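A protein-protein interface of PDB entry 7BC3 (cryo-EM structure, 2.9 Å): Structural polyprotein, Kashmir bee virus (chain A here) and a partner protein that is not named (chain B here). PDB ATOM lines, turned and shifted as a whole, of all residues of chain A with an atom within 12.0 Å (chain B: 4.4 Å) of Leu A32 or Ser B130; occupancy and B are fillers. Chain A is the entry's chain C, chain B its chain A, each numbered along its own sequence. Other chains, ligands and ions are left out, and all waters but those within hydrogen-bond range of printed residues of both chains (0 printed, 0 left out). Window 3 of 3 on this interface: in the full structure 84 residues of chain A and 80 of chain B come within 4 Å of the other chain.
The backbone carbonyl oxygen of His B131 lies within hydrogen-bond range of the backbone NH of Ser B112. OG of Ser B130 sits at hydrogen-bond distance from O of Ser B112. OD2 of Asp A27 is in hydrogen-bond range of OG of Ser A29 (3.5 Å).
N of Glu B144 sits at hydrogen-bond distance from O of Val A30. The backbone NH (N) of Leu A32 is in hydrogen-bond range of the backbone carbonyl oxygen (O) of Glu B144 (3.1 Å).
Of the printed residues of chain B, Leu A32 touches Leu B114, Pro B129, Ser B130, His B131, Val B143, Glu B144, Pro B146, Tyr B148 and Leu B168. Of chain A, only Leu A32 comes within 4 Å of Ser B130. No residue of chain A comes within 4 Å of Arg B111. Gly B128 touches none of the printed residues of chain A. Printed residues of chain A within 4 Å of Pro B129: Leu A32 (3.3 Å). His B131 touches just these residues of chain A: Val A30 (3.4 Å) and Leu A32 (3.9 Å). Of chain A, only Ser A29 (3.8 Å), Val A30 (3.4 Å) and Leu A32 (3.6 Å) come within 4 Å of Val B143. Of chain A, only Val A30 (2.7 Å), Pro A31 (3.6 Å) and Leu A32 (3.1 Å) come within 4 Å of Glu B144. Pro B146 touches just these residues of chain A: Leu A32, Ala A33 and Asn A38. Leu B168 touches just one residue of chain A: Leu A32 (3.3 Å). Of the printed residues of chain B, Asn A38 touches Pro B146. Printed residues of chain B within 4 Å of Pro A31: Glu B144. The nearest residue of chain A that does not touch Ser B130 is Val A30 (5.1 Å). The nearest printed residue of chain B that does not touch Pro A31 is Pro B129 (5.3 Å).
Of the 14 printed residues of chain A, 7 touch a printed residue of chain B. Hydrophobic or aromatic side chains of chain A within 4 Å of the printed part of chain B: Val A30, Leu A32 and Ala A33. Of the 13 printed residues of chain B, 9 touch a printed residue of chain A. Hydrophobic or aromatic side chains of chain B within 4 Å of the printed part of chain A: Leu B114, Pro B129, His B131, Val B143, Pro B146, Tyr B148 and Leu B168. Along chain B the printed residues that touch a printed residue of chain A span positions 114 to 168. Among the printed residues, 18 pairs touch across the chains. Among the printed residues, no Asp or Glu carboxylate lies within 4 Å of a Lys or Arg side-chain nitrogen of the other chain.
Among the printed residues, pairs that only touch across the chains: Ser A29 with Val B143 (3.8 Å), Val A30 with His B131 (3.4 Å), Val A30 with Val B143 (3.4 Å), Pro A31 with Glu B144 (3.6 Å), Leu A32 with Leu B114 (3.3 Å), Leu A32 with Pro B129 (3.3 Å), Leu A32 with Ser B130 (3.8 Å), Leu A32 with His B131 (3.9 Å), Leu A32 with Val B143 (3.6 Å), Leu A32 with Pro B146 (3.97 Å), Leu A32 with Tyr B148 (3.8 Å), Leu A32 with Leu B168 (3.3 Å), Ala A33 with Pro B146 (3.8 Å), Ala A33 with Tyr B148 (3.3 Å), Tyr A34 with Tyr B148 (3.6 Å) and Asn A38 with Pro B146 (3.96 Å).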
ATOM      1  N   ASP A  27      12.360  -1.004  -9.291  1.00  0.00           N
ATOM      2  CA  ASP A  27      12.469  -2.361  -8.784  1.00  0.00           C
ATOM      3  C   ASP A  27      11.946  -2.439  -7.359  1.00  0.00           C
ATOM      4  O   ASP A  27      12.233  -1.569  -6.530  1.00  0.00           O
ATOM      5  CB  ASP A  27      13.920  -2.834  -8.834  1.00  0.00           C
ATOM      6  CG  ASP A  27      14.037  -4.338  -8.971  1.00  0.00           C
ATOM      7  OD1 ASP A  27      13.006  -5.032  -8.854  1.00  0.00           O
ATOM      8  OD2 ASP A  27      15.161  -4.825  -9.204  1.00  0.00           O
ATOM      9  N   MET A  28      11.181  -3.489  -7.077  1.00  0.00           N
ATOM     10  CA  MET A  28      10.641  -3.739  -5.753  1.00  0.00           C
ATOM     11  C   MET A  28      11.547  -4.635  -4.923  1.00  0.00           C
ATOM     12  O   MET A  28      11.067  -5.323  -4.014  1.00  0.00           O
ATOM     13  CB  MET A  28       9.248  -4.352  -5.875  1.00  0.00           C
ATOM     14  CG  MET A  28       8.224  -3.398  -6.466  1.00  0.00           C
ATOM     15  SD  MET A  28       7.941  -1.948  -5.441  1.00  0.00           S
ATOM     16  CE  MET A  28       7.414  -2.736  -3.927  1.00  0.00           C
ATOM     17  N   SER A  29      12.843  -4.642  -5.218  1.00  0.00           N
ATOM     18  CA  SER A  29      13.791  -5.454  -4.473  1.00  0.00           C
ATOM     19  C   SER A  29      14.137  -4.773  -3.157  1.00  0.00           C
ATOM     20  O   SER A  29      14.482  -3.589  -3.130  1.00  0.00           O
ATOM     21  CB  SER A  29      15.054  -5.678  -5.300  1.00  0.00           C
ATOM     22  OG  SER A  29      14.844  -6.665  -6.294  1.00  0.00           O
ATOM     23  N   VAL A  30      14.043  -5.522  -2.067  1.00  0.00           N
ATOM     24  CA  VAL A  30      14.323  -4.962  -0.744  1.00  0.00           C
ATOM     25  C   VAL A  30      15.829  -4.981  -0.511  1.00  0.00           C
ATOM     26  O   VAL A  30      16.454  -6.045  -0.641  1.00  0.00           O
ATOM     27  CB  VAL A  30      13.593  -5.748   0.336  1.00  0.00           C
ATOM     28  CG1 VAL A  30      13.994  -5.248   1.704  1.00  0.00           C
ATOM     29  CG2 VAL A  30      12.096  -5.631   0.150  1.00  0.00           C
ATOM     30  N   PRO A  31      16.445  -3.849  -0.169  1.00  0.00           N
ATOM     31  CA  PRO A  31      17.888  -3.841   0.079  1.00  0.00           C
ATOM     32  C   PRO A  31      18.240  -4.255   1.499  1.00  0.00           C
ATOM     33  O   PRO A  31      17.685  -3.756   2.480  1.00  0.00           O
ATOM     34  CB  PRO A  31      18.266  -2.378  -0.180  1.00  0.00           C
ATOM     35  CG  PRO A  31      17.057  -1.617   0.184  1.00  0.00           C
ATOM     36  CD  PRO A  31      15.871  -2.494  -0.099  1.00  0.00           C
ATOM     37  N   LEU A  32      19.184  -5.186   1.597  1.00  0.00           N
ATOM     38  CA  LEU A  32      19.689  -5.650   2.887  1.00  0.00           C
ATOM     39  C   LEU A  32      20.750  -4.684   3.406  1.00  0.00           C
ATOM     40  O   LEU A  32      21.890  -5.046   3.690  1.00  0.00           O
ATOM     41  CB  LEU A  32      20.246  -7.059   2.760  1.00  0.00           C
ATOM     42  CG  LEU A  32      19.289  -8.080   2.163  1.00  0.00           C
ATOM     43  CD1 LEU A  32      20.014  -9.372   1.889  1.00  0.00           C
ATOM     44  CD2 LEU A  32      18.134  -8.297   3.104  1.00  0.00           C
ATOM     45  N   ALA A  33      20.343  -3.428   3.528  1.00  0.00           N
ATOM     46  CA  ALA A  33      21.254  -2.337   3.809  1.00  0.00           C
ATOM     47  C   ALA A  33      20.765  -1.554   5.018  1.00  0.00           C
ATOM     48  O   ALA A  33      19.816  -1.940   5.706  1.00  0.00           O
ATOM     49  CB  ALA A  33      21.391  -1.414   2.594  1.00  0.00           C
ATOM     50  N   TYR A  34      21.444  -0.441   5.261  1.00  0.00           N
ATOM     51  CA  TYR A  34      21.069   0.533   6.269  1.00  0.00           C
ATOM     52  C   TYR A  34      20.243   1.665   5.674  1.00  0.00           C
ATOM     53  O   TYR A  34      19.138   1.925   6.156  1.00  0.00           O
ATOM     54  CB  TYR A  34      22.359   1.040   6.939  1.00  0.00           C
ATOM     55  CG  TYR A  34      22.320   2.269   7.816  1.00  0.00           C
ATOM     56  CD1 TYR A  34      21.869   2.204   9.125  1.00  0.00           C
ATOM     57  CD2 TYR A  34      22.841   3.473   7.365  1.00  0.00           C
ATOM     58  CE1 TYR A  34      21.873   3.322   9.936  1.00  0.00           C
ATOM     59  CE2 TYR A  34      22.847   4.595   8.167  1.00  0.00           C
ATOM     60  CZ  TYR A  34      22.363   4.513   9.451  1.00  0.00           C
ATOM     61  OH  TYR A  34      22.373   5.629  10.253  1.00  0.00           O
ATOM     62  N   ASP A  35      20.687   2.246   4.563  1.00  0.00           N
ATOM     63  CA  ASP A  35      20.019   3.347   3.889  1.00  0.00           C
ATOM     64  C   ASP A  35      19.218   2.845   2.693  1.00  0.00           C
ATOM     65  O   ASP A  35      19.742   2.054   1.896  1.00  0.00           O
ATOM     66  CB  ASP A  35      21.060   4.381   3.425  1.00  0.00           C
ATOM     67  CG  ASP A  35      20.455   5.733   3.110  1.00  0.00           C
ATOM     68  OD1 ASP A  35      19.304   5.784   2.636  1.00  0.00           O
ATOM     69  OD2 ASP A  35      21.137   6.754   3.337  1.00  0.00           O
ATOM     70  N   PRO A  36      17.958   3.267   2.525  1.00  0.00           N
ATOM     71  CA  PRO A  36      17.259   2.942   1.273  1.00  0.00           C
ATOM     72  C   PRO A  36      17.875   3.627   0.074  1.00  0.00           C
ATOM     73  O   PRO A  36      17.777   3.110  -1.046  1.00  0.00           O
ATOM     74  CB  PRO A  36      15.824   3.431   1.518  1.00  0.00           C
ATOM     75  CG  PRO A  36      15.742   3.786   2.953  1.00  0.00           C
ATOM     76  CD  PRO A  36      17.115   4.078   3.420  1.00  0.00           C
ATOM     77  N   ASN A  37      18.506   4.780   0.277  1.00  0.00           N
ATOM     78  CA  ASN A  37      19.172   5.515  -0.783  1.00  0.00           C
ATOM     79  C   ASN A  37      20.620   5.084  -0.962  1.00  0.00           C
ATOM     80  O   ASN A  37      21.435   5.861  -1.472  1.00  0.00           O
ATOM     81  CB  ASN A  37      19.087   7.015  -0.503  1.00  0.00           C
ATOM     82  CG  ASN A  37      17.687   7.556  -0.686  1.00  0.00           C
ATOM     83  OD1 ASN A  37      16.957   7.766   0.281  1.00  0.00           O
ATOM     84  ND2 ASN A  37      17.300   7.779  -1.937  1.00  0.00           N
ATOM     85  N   ASN A  38      20.955   3.868  -0.540  1.00  0.00           N
ATOM     86  CA  ASN A  38      22.264   3.300  -0.819  1.00  0.00           C
ATOM     87  C   ASN A  38      22.562   3.369  -2.308  1.00  0.00           C
ATOM     88  O   ASN A  38      21.755   2.941  -3.139  1.00  0.00           O
ATOM     89  CB  ASN A  38      22.310   1.851  -0.335  1.00  0.00           C
ATOM     90  CG  ASN A  38      23.604   1.155  -0.691  1.00  0.00           C
ATOM     91  OD1 ASN A  38      23.901   0.925  -1.864  1.00  0.00           O
ATOM     92  ND2 ASN A  38      24.377   0.800   0.322  1.00  0.00           N
ATOM     93  N   GLU A  39      23.728   3.914  -2.644  1.00  0.00           N
ATOM     94  CA  GLU A  39      24.140   4.033  -4.034  1.00  0.00           C
ATOM     95  C   GLU A  39      25.644   4.235  -4.073  1.00  0.00           C
ATOM     96  O   GLU A  39      26.173   5.087  -3.354  1.00  0.00           O
ATOM     97  CB  GLU A  39      23.424   5.198  -4.727  1.00  0.00           C
ATOM     98  CG  GLU A  39      23.817   6.566  -4.203  1.00  0.00           C
ATOM     99  CD  GLU A  39      22.682   7.566  -4.270  1.00  0.00           C
ATOM    100  OE1 GLU A  39      21.981   7.742  -3.251  1.00  0.00           O
ATOM    101  OE2 GLU A  39      22.491   8.177  -5.341  1.00  0.00           O
ATOM    102  N   LEU A  40      26.324   3.448  -4.897  1.00  0.00           N
ATOM    103  CA  LEU A  40      27.748   3.649  -5.086  1.00  0.00           C
ATOM    104  C   LEU A  40      27.994   4.960  -5.824  1.00  0.00           C
ATOM    105  O   LEU A  40      27.078   5.579  -6.373  1.00  0.00           O
ATOM    106  CB  LEU A  40      28.361   2.491  -5.873  1.00  0.00           C
ATOM    107  CG  LEU A  40      28.643   1.177  -5.143  1.00  0.00           C
ATOM    108  CD1 LEU A  40      29.704   1.381  -4.093  1.00  0.00           C
ATOM    109  CD2 LEU A  40      27.383   0.602  -4.526  1.00  0.00           C
ATOM    110  N   ARG B 111      12.973 -16.368   4.044  1.00  0.00           N
ATOM    111  CA  ARG B 111      13.791 -15.380   4.725  1.00  0.00           C
ATOM    112  C   ARG B 111      15.171 -15.332   4.092  1.00  0.00           C
ATOM    113  O   ARG B 111      15.743 -16.370   3.748  1.00  0.00           O
ATOM    114  CB  ARG B 111      13.904 -15.706   6.211  1.00  0.00           C
ATOM    115  CG  ARG B 111      14.087 -14.503   7.082  1.00  0.00           C
ATOM    116  CD  ARG B 111      13.804 -14.843   8.517  1.00  0.00           C
ATOM    117  NE  ARG B 111      14.265 -13.788   9.406  1.00  0.00           N
ATOM    118  CZ  ARG B 111      14.577 -13.967  10.681  1.00  0.00           C
ATOM    119  NH1 ARG B 111      14.478 -15.165  11.240  1.00  0.00           N
ATOM    120  NH2 ARG B 111      14.993 -12.942  11.400  1.00  0.00           N
ATOM    121  N   SER B 112      15.697 -14.120   3.944  1.00  0.00           N
ATOM    122  CA  SER B 112      17.002 -13.896   3.342  1.00  0.00           C
ATOM    123  C   SER B 112      17.860 -13.065   4.281  1.00  0.00           C
ATOM    124  O   SER B 112      17.390 -12.084   4.866  1.00  0.00           O
ATOM    125  CB  SER B 112      16.880 -13.190   1.993  1.00  0.00           C
ATOM    126  OG  SER B 112      16.498 -11.839   2.158  1.00  0.00           O
ATOM    127  N   PHE B 113      19.121 -13.462   4.414  1.00  0.00           N
ATOM    128  CA  PHE B 113      20.080 -12.782   5.266  1.00  0.00           C
ATOM    129  C   PHE B 113      21.305 -12.409   4.445  1.00  0.00           C
ATOM    130  O   PHE B 113      21.465 -12.828   3.296  1.00  0.00           O
ATOM    131  CB  PHE B 113      20.494 -13.662   6.451  1.00  0.00           C
ATOM    132  CG  PHE B 113      19.341 -14.230   7.216  1.00  0.00           C
ATOM    133  CD1 PHE B 113      18.783 -13.529   8.269  1.00  0.00           C
ATOM    134  CD2 PHE B 113      18.814 -15.464   6.884  1.00  0.00           C
ATOM    135  CE1 PHE B 113      17.724 -14.049   8.975  1.00  0.00           C
ATOM    136  CE2 PHE B 113      17.753 -15.987   7.587  1.00  0.00           C
ATOM    137  CZ  PHE B 113      17.208 -15.278   8.635  1.00  0.00           C
ATOM    138  N   LEU B 114      22.173 -11.608   5.052  1.00  0.00           N
ATOM    139  CA  LEU B 114      23.466 -11.323   4.459  1.00  0.00           C
ATOM    140  C   LEU B 114      24.478 -12.386   4.867  1.00  0.00           C
ATOM    141  O   LEU B 114      24.267 -13.159   5.805  1.00  0.00           O
ATOM    142  CB  LEU B 114      23.972  -9.948   4.886  1.00  0.00           C
ATOM    143  CG  LEU B 114      23.414  -8.730   4.158  1.00  0.00           C
ATOM    144  CD1 LEU B 114      23.818  -7.480   4.897  1.00  0.00           C
ATOM    145  CD2 LEU B 114      23.899  -8.679   2.724  1.00  0.00           C
ATOM    146  N   GLY B 128      21.768  -8.997  11.545  1.00  0.00           N
ATOM    147  CA  GLY B 128      21.894  -8.105  10.422  1.00  0.00           C
ATOM    148  C   GLY B 128      20.561  -7.875   9.747  1.00  0.00           C
ATOM    149  O   GLY B 128      19.526  -8.400  10.167  1.00  0.00           O
ATOM    150  N   PRO B 129      20.561  -7.081   8.683  1.00  0.00           N
ATOM    151  CA  PRO B 129      19.316  -6.840   7.952  1.00  0.00           C
ATOM    152  C   PRO B 129      18.809  -8.110   7.292  1.00  0.00           C
ATOM    153  O   PRO B 129      19.577  -9.006   6.938  1.00  0.00           O
ATOM    154  CB  PRO B 129      19.704  -5.784   6.912  1.00  0.00           C
ATOM    155  CG  PRO B 129      21.182  -5.809   6.841  1.00  0.00           C
ATOM    156  CD  PRO B 129      21.697  -6.325   8.135  1.00  0.00           C
ATOM    157  N   SER B 130      17.490  -8.174   7.130  1.00  0.00           N
ATOM    158  CA  SER B 130      16.846  -9.358   6.589  1.00  0.00           C
ATOM    159  C   SER B 130      15.592  -8.947   5.838  1.00  0.00           C
ATOM    160  O   SER B 130      15.085  -7.834   5.992  1.00  0.00           O
ATOM    161  CB  SER B 130      16.495 -10.361   7.693  1.00  0.00           C
ATOM    162  OG  SER B 130      15.932 -11.541   7.148  1.00  0.00           O
ATOM    163  N   HIS B 131      15.100  -9.869   5.018  1.00  0.00           N
ATOM    164  CA  HIS B 131      13.845  -9.709   4.302  1.00  0.00           C
ATOM    165  C   HIS B 131      13.068 -11.009   4.395  1.00  0.00           C
ATOM    166  O   HIS B 131      13.630 -12.092   4.207  1.00  0.00           O
ATOM    167  CB  HIS B 131      14.069  -9.339   2.837  1.00  0.00           C
ATOM    168  CG  HIS B 131      12.803  -9.099   2.079  1.00  0.00           C
ATOM    169  ND1 HIS B 131      12.603  -9.564   0.797  1.00  0.00           N
ATOM    170  CD2 HIS B 131      11.667  -8.449   2.424  1.00  0.00           C
ATOM    171  CE1 HIS B 131      11.400  -9.207   0.385  1.00  0.00           C
ATOM    172  NE2 HIS B 131      10.811  -8.531   1.354  1.00  0.00           N
ATOM    173  N   VAL B 143      14.945  -9.289  -3.472  1.00  0.00           N
ATOM    174  CA  VAL B 143      15.939  -8.819  -2.518  1.00  0.00           C
ATOM    175  C   VAL B 143      17.130  -8.255  -3.279  1.00  0.00           C
ATOM    176  O   VAL B 143      17.429  -8.669  -4.402  1.00  0.00           O
ATOM    177  CB  VAL B 143      16.382  -9.944  -1.559  1.00  0.00           C
ATOM    178  CG1 VAL B 143      17.189 -10.996  -2.298  1.00  0.00           C
ATOM    179  CG2 VAL B 143      17.169  -9.373  -0.399  1.00  0.00           C
ATOM    180  N   GLU B 144      17.811  -7.302  -2.650  1.00  0.00           N
ATOM    181  CA  GLU B 144      18.986  -6.661  -3.216  1.00  0.00           C
ATOM    182  C   GLU B 144      20.139  -6.762  -2.231  1.00  0.00           C
ATOM    183  O   GLU B 144      19.953  -6.586  -1.024  1.00  0.00           O
ATOM    184  CB  GLU B 144      18.711  -5.194  -3.546  1.00  0.00           C
ATOM    185  CG  GLU B 144      19.902  -4.452  -4.115  1.00  0.00           C
ATOM    186  CD  GLU B 144      19.582  -3.011  -4.433  1.00  0.00           C
ATOM    187  OE1 GLU B 144      18.412  -2.612  -4.260  1.00  0.00           O
ATOM    188  OE2 GLU B 144      20.499  -2.274  -4.852  1.00  0.00           O
ATOM    189  N   PRO B 146      23.807  -5.108  -1.395  1.00  0.00           N
ATOM    190  CA  PRO B 146      24.682  -3.981  -1.722  1.00  0.00           C
ATOM    191  C   PRO B 146      26.118  -4.445  -1.930  1.00  0.00           C
ATOM    192  O   PRO B 146      26.448  -5.623  -1.810  1.00  0.00           O
ATOM    193  CB  PRO B 146      24.566  -3.069  -0.496  1.00  0.00           C
ATOM    194  CG  PRO B 146      23.396  -3.563   0.262  1.00  0.00           C
ATOM    195  CD  PRO B 146      23.328  -5.017  -0.008  1.00  0.00           C
ATOM    196  N   TYR B 148      29.031  -4.283  -0.184  1.00  0.00           N
ATOM    197  CA  TYR B 148      29.753  -4.161   1.079  1.00  0.00           C
ATOM    198  C   TYR B 148      31.098  -4.847   0.908  1.00  0.00           C
ATOM    199  O   TYR B 148      31.215  -6.061   1.068  1.00  0.00           O
ATOM    200  CB  TYR B 148      28.954  -4.780   2.218  1.00  0.00           C
ATOM    201  CG  TYR B 148      27.759  -3.970   2.654  1.00  0.00           C
ATOM    202  CD1 TYR B 148      27.846  -2.597   2.805  1.00  0.00           C
ATOM    203  CD2 TYR B 148      26.547  -4.582   2.921  1.00  0.00           C
ATOM    204  CE1 TYR B 148      26.760  -1.857   3.205  1.00  0.00           C
ATOM    205  CE2 TYR B 148      25.454  -3.851   3.325  1.00  0.00           C
ATOM    206  CZ  TYR B 148      25.566  -2.488   3.463  1.00  0.00           C
ATOM    207  OH  TYR B 148      24.481  -1.753   3.866  1.00  0.00           O
ATOM    208  N   LEU B 168      24.429 -13.410  -0.236  1.00  0.00           N
ATOM    209  CA  LEU B 168      23.091 -13.683   0.261  1.00  0.00           C
ATOM    210  C   LEU B 168      23.032 -15.052   0.916  1.00  0.00           C
ATOM    211  O   LEU B 168      23.616 -16.019   0.417  1.00  0.00           O
ATOM    212  CB  LEU B 168      22.070 -13.615  -0.869  1.00  0.00           C
ATOM    213  CG  LEU B 168      20.627 -13.498  -0.392  1.00  0.00           C
ATOM    214  CD1 LEU B 168      20.311 -12.058  -0.057  1.00  0.00           C
ATOM    215  CD2 LEU B 168      19.679 -14.039  -1.438  1.00  0.00           C
